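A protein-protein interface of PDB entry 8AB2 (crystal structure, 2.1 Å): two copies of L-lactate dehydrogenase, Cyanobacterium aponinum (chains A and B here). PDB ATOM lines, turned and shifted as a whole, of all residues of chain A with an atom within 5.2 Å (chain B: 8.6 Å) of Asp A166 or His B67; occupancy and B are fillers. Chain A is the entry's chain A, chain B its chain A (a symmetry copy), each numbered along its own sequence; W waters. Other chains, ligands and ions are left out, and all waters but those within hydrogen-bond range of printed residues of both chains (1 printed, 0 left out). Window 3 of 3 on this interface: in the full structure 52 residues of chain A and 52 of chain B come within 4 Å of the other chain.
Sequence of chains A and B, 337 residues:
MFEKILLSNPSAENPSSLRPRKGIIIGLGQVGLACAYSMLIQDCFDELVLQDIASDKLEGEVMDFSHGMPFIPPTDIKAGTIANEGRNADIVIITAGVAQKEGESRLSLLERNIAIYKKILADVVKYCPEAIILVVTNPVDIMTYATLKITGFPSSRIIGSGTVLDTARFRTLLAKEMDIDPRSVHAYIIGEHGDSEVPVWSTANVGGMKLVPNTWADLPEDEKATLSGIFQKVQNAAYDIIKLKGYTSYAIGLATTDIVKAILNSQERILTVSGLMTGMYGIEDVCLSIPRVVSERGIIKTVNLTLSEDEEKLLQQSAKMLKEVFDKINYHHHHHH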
ATOM      1  N   THR A 163     -13.069  26.362   4.307  1.00  0.00           N
ATOM      2  CA  THR A 163     -13.017  27.004   5.614  1.00  0.00           C
ATOM      3  C   THR A 163     -14.174  27.973   5.835  1.00  0.00           C
ATOM      4  O   THR A 163     -14.082  28.846   6.705  1.00  0.00           O
ATOM      5  CB  THR A 163     -11.687  27.738   5.791  1.00  0.00           C
ATOM      6  OG1 THR A 163     -11.598  28.802   4.835  1.00  0.00           O
ATOM      7  CG2 THR A 163     -10.517  26.785   5.590  1.00  0.00           C
ATOM      8  N   VAL A 164     -15.257  27.839   5.064  1.00  0.00           N
ATOM      9  CA  VAL A 164     -16.399  28.740   5.208  1.00  0.00           C
ATOM     10  C   VAL A 164     -16.927  28.714   6.637  1.00  0.00           C
ATOM     11  O   VAL A 164     -17.262  29.760   7.210  1.00  0.00           O
ATOM     12  CB  VAL A 164     -17.495  28.372   4.191  1.00  0.00           C
ATOM     13  CG1 VAL A 164     -18.777  29.139   4.480  1.00  0.00           C
ATOM     14  CG2 VAL A 164     -17.016  28.650   2.778  1.00  0.00           C
ATOM     15  N   LEU A 165     -16.992  27.525   7.240  1.00  0.00           N
ATOM     16  CA  LEU A 165     -17.525  27.397   8.593  1.00  0.00           C
ATOM     17  C   LEU A 165     -16.641  28.113   9.610  1.00  0.00           C
ATOM     18  O   LEU A 165     -17.132  28.903  10.425  1.00  0.00           O
ATOM     19  CB  LEU A 165     -17.675  25.919   8.953  1.00  0.00           C
ATOM     20  CG  LEU A 165     -18.006  25.570  10.406  1.00  0.00           C
ATOM     21  CD1 LEU A 165     -19.273  26.274  10.867  1.00  0.00           C
ATOM     22  CD2 LEU A 165     -18.140  24.063  10.566  1.00  0.00           C
ATOM     23  N   ASP A 166     -15.334  27.847   9.581  1.00  0.00           N
ATOM     24  CA  ASP A 166     -14.442  28.460  10.561  1.00  0.00           C
ATOM     25  C   ASP A 166     -14.299  29.961  10.338  1.00  0.00           C
ATOM     26  O   ASP A 166     -14.152  30.717  11.306  1.00  0.00           O
ATOM     27  CB  ASP A 166     -13.076  27.774  10.528  1.00  0.00           C
ATOM     28  CG  ASP A 166     -13.130  26.349  11.051  1.00  0.00           C
ATOM     29  OD1 ASP A 166     -14.170  25.967  11.628  1.00  0.00           O
ATOM     30  OD2 ASP A 166     -12.140  25.609  10.883  1.00  0.00           O
ATOM     31  N   THR A 167     -14.344  30.413   9.081  1.00  0.00           N
ATOM     32  CA  THR A 167     -14.277  31.846   8.808  1.00  0.00           C
ATOM     33  C   THR A 167     -15.472  32.578   9.405  1.00  0.00           C
ATOM     34  O   THR A 167     -15.323  33.666   9.976  1.00  0.00           O
ATOM     35  CB  THR A 167     -14.189  32.089   7.299  1.00  0.00           C
ATOM     36  OG1 THR A 167     -12.875  31.754   6.833  1.00  0.00           O
ATOM     37  CG2 THR A 167     -14.485  33.545   6.963  1.00  0.00           C
ATOM     38  N   ALA A 168     -16.667  31.992   9.298  1.00  0.00           N
ATOM     39  CA  ALA A 168     -17.856  32.634   9.853  1.00  0.00           C
ATOM     40  C   ALA A 168     -17.772  32.731  11.371  1.00  0.00           C
ATOM     41  O   ALA A 168     -18.139  33.759  11.955  1.00  0.00           O
ATOM     42  CB  ALA A 168     -19.113  31.873   9.430  1.00  0.00           C
ATOM     43  N   ARG A 169     -17.294  31.672  12.030  1.00  0.00           N
ATOM     44  CA  ARG A 169     -17.098  31.735  13.475  1.00  0.00           C
ATOM     45  C   ARG A 169     -16.015  32.744  13.834  1.00  0.00           C
ATOM     46  O   ARG A 169     -16.160  33.506  14.797  1.00  0.00           O
ATOM     47  CB  ARG A 169     -16.741  30.352  14.019  1.00  0.00           C
ATOM     48  CG  ARG A 169     -16.774  30.258  15.536  1.00  0.00           C
ATOM     49  CD  ARG A 169     -18.206  30.182  16.046  1.00  0.00           C
ATOM     50  NE  ARG A 169     -18.286  30.325  17.495  1.00  0.00           N
ATOM     51  CZ  ARG A 169     -18.088  29.340  18.361  1.00  0.00           C
ATOM     52  NH1 ARG A 169     -17.769  28.120  17.960  1.00  0.00           N
ATOM     53  NH2 ARG A 169     -18.211  29.585  19.663  1.00  0.00           N
ATOM     54  N   PHE A 170     -14.922  32.755  13.068  1.00  0.00           N
ATOM     55  CA  PHE A 170     -13.866  33.745  13.257  1.00  0.00           C
ATOM     56  C   PHE A 170     -14.423  35.159  13.147  1.00  0.00           C
ATOM     57  O   PHE A 170     -14.157  36.016  13.998  1.00  0.00           O
ATOM     58  CB  PHE A 170     -12.767  33.503  12.220  1.00  0.00           C
ATOM     59  CG  PHE A 170     -11.523  34.315  12.431  1.00  0.00           C
ATOM     60  CD1 PHE A 170     -10.914  34.374  13.673  1.00  0.00           C
ATOM     61  CD2 PHE A 170     -10.938  34.987  11.371  1.00  0.00           C
ATOM     62  CE1 PHE A 170      -9.757  35.112  13.858  1.00  0.00           C
ATOM     63  CE2 PHE A 170      -9.782  35.724  11.547  1.00  0.00           C
ATOM     64  CZ  PHE A 170      -9.191  35.786  12.791  1.00  0.00           C
ATOM     65  N   ARG A 171     -15.221  35.410  12.106  1.00  0.00           N
ATOM     66  CA  ARG A 171     -15.814  36.731  11.919  1.00  0.00           C
ATOM     67  C   ARG A 171     -16.744  37.092  13.070  1.00  0.00           C
ATOM     68  O   ARG A 171     -16.724  38.225  13.564  1.00  0.00           O
ATOM     69  CB  ARG A 171     -16.569  36.769  10.590  1.00  0.00           C
ATOM     70  CG  ARG A 171     -17.309  38.067  10.319  1.00  0.00           C
ATOM     71  CD  ARG A 171     -18.288  37.893   9.169  1.00  0.00           C
ATOM     72  NE  ARG A 171     -18.339  39.071   8.310  1.00  0.00           N
ATOM     73  CZ  ARG A 171     -19.116  39.186   7.243  1.00  0.00           C
ATOM     74  NH1 ARG A 171     -19.942  38.217   6.881  1.00  0.00           N
ATOM     75  NH2 ARG A 171     -19.063  40.299   6.519  1.00  0.00           N
ATOM     76  N   ILE A 189     -10.231  33.064   7.092  1.00  0.00           N
ATOM     77  CA  ILE A 189      -9.400  31.901   7.375  1.00  0.00           C
ATOM     78  C   ILE A 189      -9.214  31.163   6.058  1.00  0.00           C
ATOM     79  O   ILE A 189     -10.195  30.737   5.435  1.00  0.00           O
ATOM     80  CB  ILE A 189     -10.030  30.994   8.442  1.00  0.00           C
ATOM     81  CG1 ILE A 189      -9.972  31.668   9.815  1.00  0.00           C
ATOM     82  CG2 ILE A 189      -9.340  29.643   8.467  1.00  0.00           C
ATOM     83  CD1 ILE A 189     -10.602  30.849  10.922  1.00  0.00           C
ATOM     84  N   HIS A 193      -8.135  23.140   5.025  1.00  0.00           N
ATOM     85  CA  HIS A 193      -9.099  22.955   6.103  1.00  0.00           C
ATOM     86  C   HIS A 193      -8.549  21.973   7.129  1.00  0.00           C
ATOM     87  O   HIS A 193      -8.272  20.813   6.805  1.00  0.00           O
ATOM     88  CB  HIS A 193     -10.431  22.462   5.546  1.00  0.00           C
ATOM     89  CG  HIS A 193     -11.452  22.166   6.601  1.00  0.00           C
ATOM     90  ND1 HIS A 193     -12.032  20.924   6.748  1.00  0.00           N
ATOM     91  CD2 HIS A 193     -11.991  22.949   7.566  1.00  0.00           C
ATOM     92  CE1 HIS A 193     -12.887  20.957   7.754  1.00  0.00           C
ATOM     93  NE2 HIS A 193     -12.881  22.174   8.268  1.00  0.00           N
ATOM     94  N   GLU A 197      -4.988  25.655   8.862  1.00  0.00           N
ATOM     95  CA  GLU A 197      -5.613  26.787   8.192  1.00  0.00           C
ATOM     96  C   GLU A 197      -5.071  28.098   8.755  1.00  0.00           C
ATOM     97  O   GLU A 197      -4.724  28.197   9.934  1.00  0.00           O
ATOM     98  CB  GLU A 197      -7.132  26.723   8.340  1.00  0.00           C
ATOM     99  CG  GLU A 197      -7.618  26.734   9.776  1.00  0.00           C
ATOM    100  CD  GLU A 197      -9.088  26.382   9.896  1.00  0.00           C
ATOM    101  OE1 GLU A 197      -9.569  25.538   9.110  1.00  0.00           O
ATOM    102  OE2 GLU A 197      -9.763  26.953  10.775  1.00  0.00           O
ATOM    103  N   VAL A 234     -11.570  29.298  17.777  1.00  0.00           N
ATOM    104  CA  VAL A 234     -12.170  28.704  16.587  1.00  0.00           C
ATOM    105  C   VAL A 234     -11.616  27.304  16.354  1.00  0.00           C
ATOM    106  O   VAL A 234     -12.363  26.359  16.075  1.00  0.00           O
ATOM    107  CB  VAL A 234     -11.946  29.611  15.362  1.00  0.00           C
ATOM    108  CG1 VAL A 234     -12.408  28.914  14.088  1.00  0.00           C
ATOM    109  CG2 VAL A 234     -12.674  30.932  15.542  1.00  0.00           C
ATOM    110  N   ALA A 237     -12.868  24.779  18.962  1.00  0.00           N
ATOM    111  CA  ALA A 237     -14.248  24.352  18.759  1.00  0.00           C
ATOM    112  C   ALA A 237     -14.341  23.255  17.708  1.00  0.00           C
ATOM    113  O   ALA A 237     -15.049  22.260  17.903  1.00  0.00           O
ATOM    114  CB  ALA A 237     -15.117  25.547  18.369  1.00  0.00           C
ATOM    115  N   ALA A 238     -13.631  23.414  16.588  1.00  0.00           N
ATOM    116  CA  ALA A 238     -13.679  22.407  15.532  1.00  0.00           C
ATOM    117  C   ALA A 238     -13.073  21.089  15.995  1.00  0.00           C
ATOM    118  O   ALA A 238     -13.565  20.012  15.637  1.00  0.00           O
ATOM    119  CB  ALA A 238     -12.965  22.920  14.283  1.00  0.00           C
ATOM    120  N   ILE A 241     -15.486  19.300  18.750  1.00  0.00           N
ATOM    121  CA  ILE A 241     -16.666  18.655  18.178  1.00  0.00           C
ATOM    122  C   ILE A 241     -16.322  17.245  17.715  1.00  0.00           C
ATOM    123  O   ILE A 241     -17.070  16.292  17.962  1.00  0.00           O
ATOM    124  CB  ILE A 241     -17.242  19.506  17.030  1.00  0.00           C
ATOM    125  CG1 ILE A 241     -17.794  20.827  17.567  1.00  0.00           C
ATOM    126  CG2 ILE A 241     -18.333  18.745  16.292  1.00  0.00           C
ATOM    127  CD1 ILE A 241     -18.192  21.801  16.482  1.00  0.00           C
ATOM    128  N   ALA A 251     -23.125  22.015  12.306  1.00  0.00           N
ATOM    129  CA  ALA A 251     -22.344  23.179  11.898  1.00  0.00           C
ATOM    130  C   ALA A 251     -22.033  23.136  10.407  1.00  0.00           C
ATOM    131  O   ALA A 251     -22.258  24.117   9.687  1.00  0.00           O
ATOM    132  CB  ALA A 251     -21.056  23.266  12.717  1.00  0.00           C
ATOM    133  N   LEU B  40     -33.481  26.346  16.502  1.00  0.00           N
ATOM    134  CA  LEU B  40     -32.351  27.250  16.316  1.00  0.00           C
ATOM    135  C   LEU B  40     -32.413  27.924  14.950  1.00  0.00           C
ATOM    136  O   LEU B  40     -32.247  29.146  14.841  1.00  0.00           O
ATOM    137  CB  LEU B  40     -31.035  26.489  16.481  1.00  0.00           C
ATOM    138  CG  LEU B  40     -30.667  26.046  17.897  1.00  0.00           C
ATOM    139  CD1 LEU B  40     -29.490  25.084  17.867  1.00  0.00           C
ATOM    140  CD2 LEU B  40     -30.351  27.251  18.766  1.00  0.00           C
ATOM    141  N   GLY B  60     -20.931  17.645  22.910  1.00  0.00           N
ATOM    142  CA  GLY B  60     -20.526  17.711  21.516  1.00  0.00           C
ATOM    143  C   GLY B  60     -21.627  18.233  20.612  1.00  0.00           C
ATOM    144  O   GLY B  60     -21.366  18.999  19.680  1.00  0.00           O
ATOM    145  N   GLU B  61     -22.871  17.818  20.867  1.00  0.00           N
ATOM    146  CA  GLU B  61     -23.997  18.361  20.114  1.00  0.00           C
ATOM    147  C   GLU B  61     -24.140  19.859  20.351  1.00  0.00           C
ATOM    148  O   GLU B  61     -24.343  20.628  19.405  1.00  0.00           O
ATOM    149  CB  GLU B  61     -25.292  17.636  20.494  1.00  0.00           C
ATOM    150  CG  GLU B  61     -25.271  16.117  20.341  1.00  0.00           C
ATOM    151  CD  GLU B  61     -25.232  15.663  18.897  1.00  0.00           C
ATOM    152  OE1 GLU B  61     -25.344  16.520  17.998  1.00  0.00           O
ATOM    153  OE2 GLU B  61     -25.093  14.446  18.656  1.00  0.00           O
ATOM    154  N   VAL B  62     -24.035  20.292  21.612  1.00  0.00           N
ATOM    155  CA  VAL B  62     -24.140  21.715  21.930  1.00  0.00           C
ATOM    156  C   VAL B  62     -23.037  22.501  21.234  1.00  0.00           C
ATOM    157  O   VAL B  62     -23.278  23.578  20.673  1.00  0.00           O
ATOM    158  CB  VAL B  62     -24.107  21.922  23.457  1.00  0.00           C
ATOM    159  CG1 VAL B  62     -23.932  23.396  23.799  1.00  0.00           C
ATOM    160  CG2 VAL B  62     -25.373  21.377  24.098  1.00  0.00           C
ATOM    161  N   MET B  63     -21.810  21.980  21.258  1.00  0.00           N
ATOM    162  CA  MET B  63     -20.716  22.668  20.585  1.00  0.00           C
ATOM    163  C   MET B  63     -20.884  22.633  19.072  1.00  0.00           C
ATOM    164  O   MET B  63     -20.486  23.580  18.383  1.00  0.00           O
ATOM    165  CB  MET B  63     -19.380  22.052  20.994  1.00  0.00           C
ATOM    166  CG  MET B  63     -18.240  23.049  21.022  1.00  0.00           C
ATOM    167  SD  MET B  63     -16.773  22.395  21.828  1.00  0.00           S
ATOM    168  CE  MET B  63     -17.430  21.961  23.435  1.00  0.00           C
ATOM    169  N   ASP B  64     -21.469  21.556  18.539  1.00  0.00           N
ATOM    170  CA  ASP B  64     -21.793  21.520  17.117  1.00  0.00           C
ATOM    171  C   ASP B  64     -22.816  22.595  16.770  1.00  0.00           C
ATOM    172  O   ASP B  64     -22.663  23.313  15.775  1.00  0.00           O
ATOM    173  CB  ASP B  64     -22.314  20.132  16.738  1.00  0.00           C
ATOM    174  CG  ASP B  64     -22.170  19.836  15.258  1.00  0.00           C
ATOM    175  OD1 ASP B  64     -21.610  20.681  14.529  1.00  0.00           O
ATOM    176  OD2 ASP B  64     -22.612  18.753  14.823  1.00  0.00           O
ATOM    177  N   PHE B  65     -23.864  22.724  17.588  1.00  0.00           N
ATOM    178  CA  PHE B  65     -24.838  23.795  17.399  1.00  0.00           C
ATOM    179  C   PHE B  65     -24.176  25.163  17.507  1.00  0.00           C
ATOM    180  O   PHE B  65     -24.391  26.040  16.664  1.00  0.00           O
ATOM    181  CB  PHE B  65     -25.964  23.668  18.428  1.00  0.00           C
ATOM    182  CG  PHE B  65     -26.935  22.550  18.147  1.00  0.00           C
ATOM    183  CD1 PHE B  65     -27.414  22.331  16.867  1.00  0.00           C
ATOM    184  CD2 PHE B  65     -27.372  21.726  19.171  1.00  0.00           C
ATOM    185  CE1 PHE B  65     -28.313  21.308  16.613  1.00  0.00           C
ATOM    186  CE2 PHE B  65     -28.268  20.701  18.925  1.00  0.00           C
ATOM    187  CZ  PHE B  65     -28.738  20.492  17.644  1.00  0.00           C
ATOM    188  N   SER B  66     -23.358  25.359  18.546  1.00  0.00           N
ATOM    189  CA  SER B  66     -22.749  26.666  18.780  1.00  0.00           C
ATOM    190  C   SER B  66     -21.829  27.070  17.635  1.00  0.00           C
ATOM    191  O   SER B  66     -21.755  28.251  17.277  1.00  0.00           O
ATOM    192  CB  SER B  66     -21.977  26.655  20.101  1.00  0.00           C
ATOM    193  OG  SER B  66     -22.831  26.373  21.193  1.00  0.00           O
ATOM    194  N   HIS B  67     -21.121  26.104  17.045  1.00  0.00           N
ATOM    195  CA  HIS B  67     -20.164  26.436  15.995  1.00  0.00           C
ATOM    196  C   HIS B  67     -20.860  26.843  14.701  1.00  0.00           C
ATOM    197  O   HIS B  67     -20.289  27.599  13.906  1.00  0.00           O
ATOM    198  CB  HIS B  67     -19.222  25.254  15.752  1.00  0.00           C
ATOM    199  CG  HIS B  67     -17.974  25.615  15.008  1.00  0.00           C
ATOM    200  ND1 HIS B  67     -17.201  26.709  15.338  1.00  0.00           N
ATOM    201  CD2 HIS B  67     -17.359  25.023  13.959  1.00  0.00           C
ATOM    202  CE1 HIS B  67     -16.167  26.777  14.519  1.00  0.00           C
ATOM    203  NE2 HIS B  67     -16.239  25.766  13.672  1.00  0.00           N
ATOM    204  N   GLY B  68     -22.085  26.367  14.474  1.00  0.00           N
ATOM    205  CA  GLY B  68     -22.824  26.738  13.282  1.00  0.00           C
ATOM    206  C   GLY B  68     -23.729  27.940  13.427  1.00  0.00           C
ATOM    207  O   GLY B  68     -24.298  28.393  12.431  1.00  0.00           O
ATOM    208  N   MET B  69     -23.859  28.469  14.644  1.00  0.00           N
ATOM    209  CA  MET B  69     -24.747  29.606  14.884  1.00  0.00           C
ATOM    210  C   MET B  69     -24.492  30.822  13.993  1.00  0.00           C
ATOM    211  O   MET B  69     -25.476  31.491  13.632  1.00  0.00           O
ATOM    212  CB  MET B  69     -24.671  30.016  16.361  1.00  0.00           C
ATOM    213  CG  MET B  69     -25.268  29.011  17.333  1.00  0.00           C
ATOM    214  SD  MET B  69     -26.989  28.606  16.977  1.00  0.00           S
ATOM    215  CE  MET B  69     -27.726  30.235  16.937  1.00  0.00           C
ATOM    216  N   PRO B  70     -23.237  31.188  13.624  1.00  0.00           N
ATOM    217  CA  PRO B  70     -23.044  32.384  12.786  1.00  0.00           C
ATOM    218  C   PRO B  70     -23.876  32.432  11.509  1.00  0.00           C
ATOM    219  O   PRO B  70     -24.105  33.517  10.966  1.00  0.00           O
ATOM    220  CB  PRO B  70     -21.547  32.330  12.460  1.00  0.00           C
ATOM    221  CG  PRO B  70     -20.949  31.719  13.660  1.00  0.00           C
ATOM    222  CD  PRO B  70     -21.945  30.690  14.138  1.00  0.00           C
ATOM    223  N   PHE B  71     -24.336  31.283  11.019  1.00  0.00           N
ATOM    224  CA  PHE B  71     -25.097  31.243   9.777  1.00  0.00           C
ATOM    225  C   PHE B  71     -26.591  31.475   9.969  1.00  0.00           C
ATOM    226  O   PHE B  71     -27.310  31.611   8.973  1.00  0.00           O
ATOM    227  CB  PHE B  71     -24.878  29.902   9.071  1.00  0.00           C
ATOM    228  CG  PHE B  71     -23.450  29.655   8.679  1.00  0.00           C
ATOM    229  CD1 PHE B  71     -22.903  30.293   7.579  1.00  0.00           C
ATOM    230  CD2 PHE B  71     -22.655  28.791   9.413  1.00  0.00           C
ATOM    231  CE1 PHE B  71     -21.589  30.070   7.212  1.00  0.00           C
ATOM    232  CE2 PHE B  71     -21.340  28.566   9.053  1.00  0.00           C
ATOM    233  CZ  PHE B  71     -20.807  29.206   7.951  1.00  0.00           C
ATOM    234  N   ILE B  72     -27.070  31.530  11.207  1.00  0.00           N
ATOM    235  CA  ILE B  72     -28.492  31.721  11.494  1.00  0.00           C
ATOM    236  C   ILE B  72     -28.622  32.839  12.524  1.00  0.00           C
ATOM    237  O   ILE B  72     -27.596  33.320  13.028  1.00  0.00           O
ATOM    238  CB  ILE B  72     -29.136  30.410  11.977  1.00  0.00           C
ATOM    239  CG1 ILE B  72     -28.350  29.819  13.150  1.00  0.00           C
ATOM    240  CG2 ILE B  72     -29.243  29.411  10.833  1.00  0.00           C
ATOM    241  CD1 ILE B  72     -28.967  28.554  13.713  1.00  0.00           C
ATOM    242  N   ILE B  77     -27.355  29.106  22.942  1.00  0.00           N
ATOM    243  CA  ILE B  77     -27.542  27.668  23.104  1.00  0.00           C
ATOM    244  C   ILE B  77     -26.509  27.146  24.092  1.00  0.00           C
ATOM    245  O   ILE B  77     -25.343  27.560  24.075  1.00  0.00           O
ATOM    246  CB  ILE B  77     -27.447  26.944  21.744  1.00  0.00           C
ATOM    247  CG1 ILE B  77     -27.673  25.438  21.912  1.00  0.00           C
ATOM    248  CG2 ILE B  77     -26.110  27.222  21.060  1.00  0.00           C
ATOM    249  CD1 ILE B  77     -29.082  25.075  22.317  1.00  0.00           C
HETATM  250  O   HOH W   1     -18.455  25.520  19.047  1.00  0.00           O
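The backbone NH (N) of Ala A251 lies within hydrogen-bond range of the side-chain carboxylate (OD1) of Asp B64 (3.0 Å). The side-chain carboxylate (OD1) of Asp A166 is in hydrogen-bond range of a ring nitrogen (NE2) of His B67 (2.9 Å). NH1 of Arg A169 is in hydrogen-bond range of ND1 of His B67, at 3.0 Å.
The side-chain carboxylate of Asp A166 lies close to the side-chain carboxylate of Glu A197 (2.7 Å). The side-chain hydroxyl (OG) of Ser B66 lies within hydrogen-bond range of the backbone carbonyl oxygen (O) of Val B62, at 2.9 Å.
No position is printed for both chains.
Among the printed residues, merely in contact across the chains: Val A164 with Phe B71, Leu A165 with His B67, Leu A165 with Phe B71, Ala A168 with Pro B70, Ala A168 with Phe B71, Arg A169 with Ser B66, Arg A169 with Pro B70, Ala A237 with His B67, Ile A241 with Met B63, Ile A241 with Asp B64, Ile A241 with His B67 and Ala A251 with Gly B68.
Water W1 lies within hydrogen-bond range of O of Met B63, NH1 of Arg A169 and N of His B67.
Of the 17 printed residues of chain A, 8 touch a printed residue of chain B. Printed residues of chain A that touch a printed residue of chain B: Val A164, Leu A165, Asp A166, Ala A168, Arg A169, Ala A237, Ile A241 and Ala A251. Along chain A the printed residues that touch a printed residue of chain B span positions 164 to 251. Among the printed residues, 15 pairs touch across the chains. Among the printed residues, no Asp or Glu carboxylate lies within 4 Å of a Lys or Arg side-chain nitrogen of the other chain.
Of the printed residues of chain B, Asp A166 touches His B67. Of chain A, only Leu A165 (3.5 Å), Asp A166 (2.9 Å), Arg A169 (3.0 Å), Ala A237 (3.9 Å) and Ile A241 (3.7 Å) come within 4 Å of His B67. Leu A165 touches two residues of chain B. Printed residues of chain A within 4 Å of Pro B70: Ala A168 and Arg A169. Printed residues of chain B within 4 Å of Ala A168: Pro B70 and Phe B71. Of the printed residues of chain B, Val A164 touches Phe B71. Leu B40 touches none of the printed residues of chain A. Val A234 touches none of the printed residues of chain B. The nearest residue of chain B that does not touch Asp A166 is Phe B71 (5.9 Å). The nearest residue of chain A that does not touch His B67 is Ala A251 (4.1 Å).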
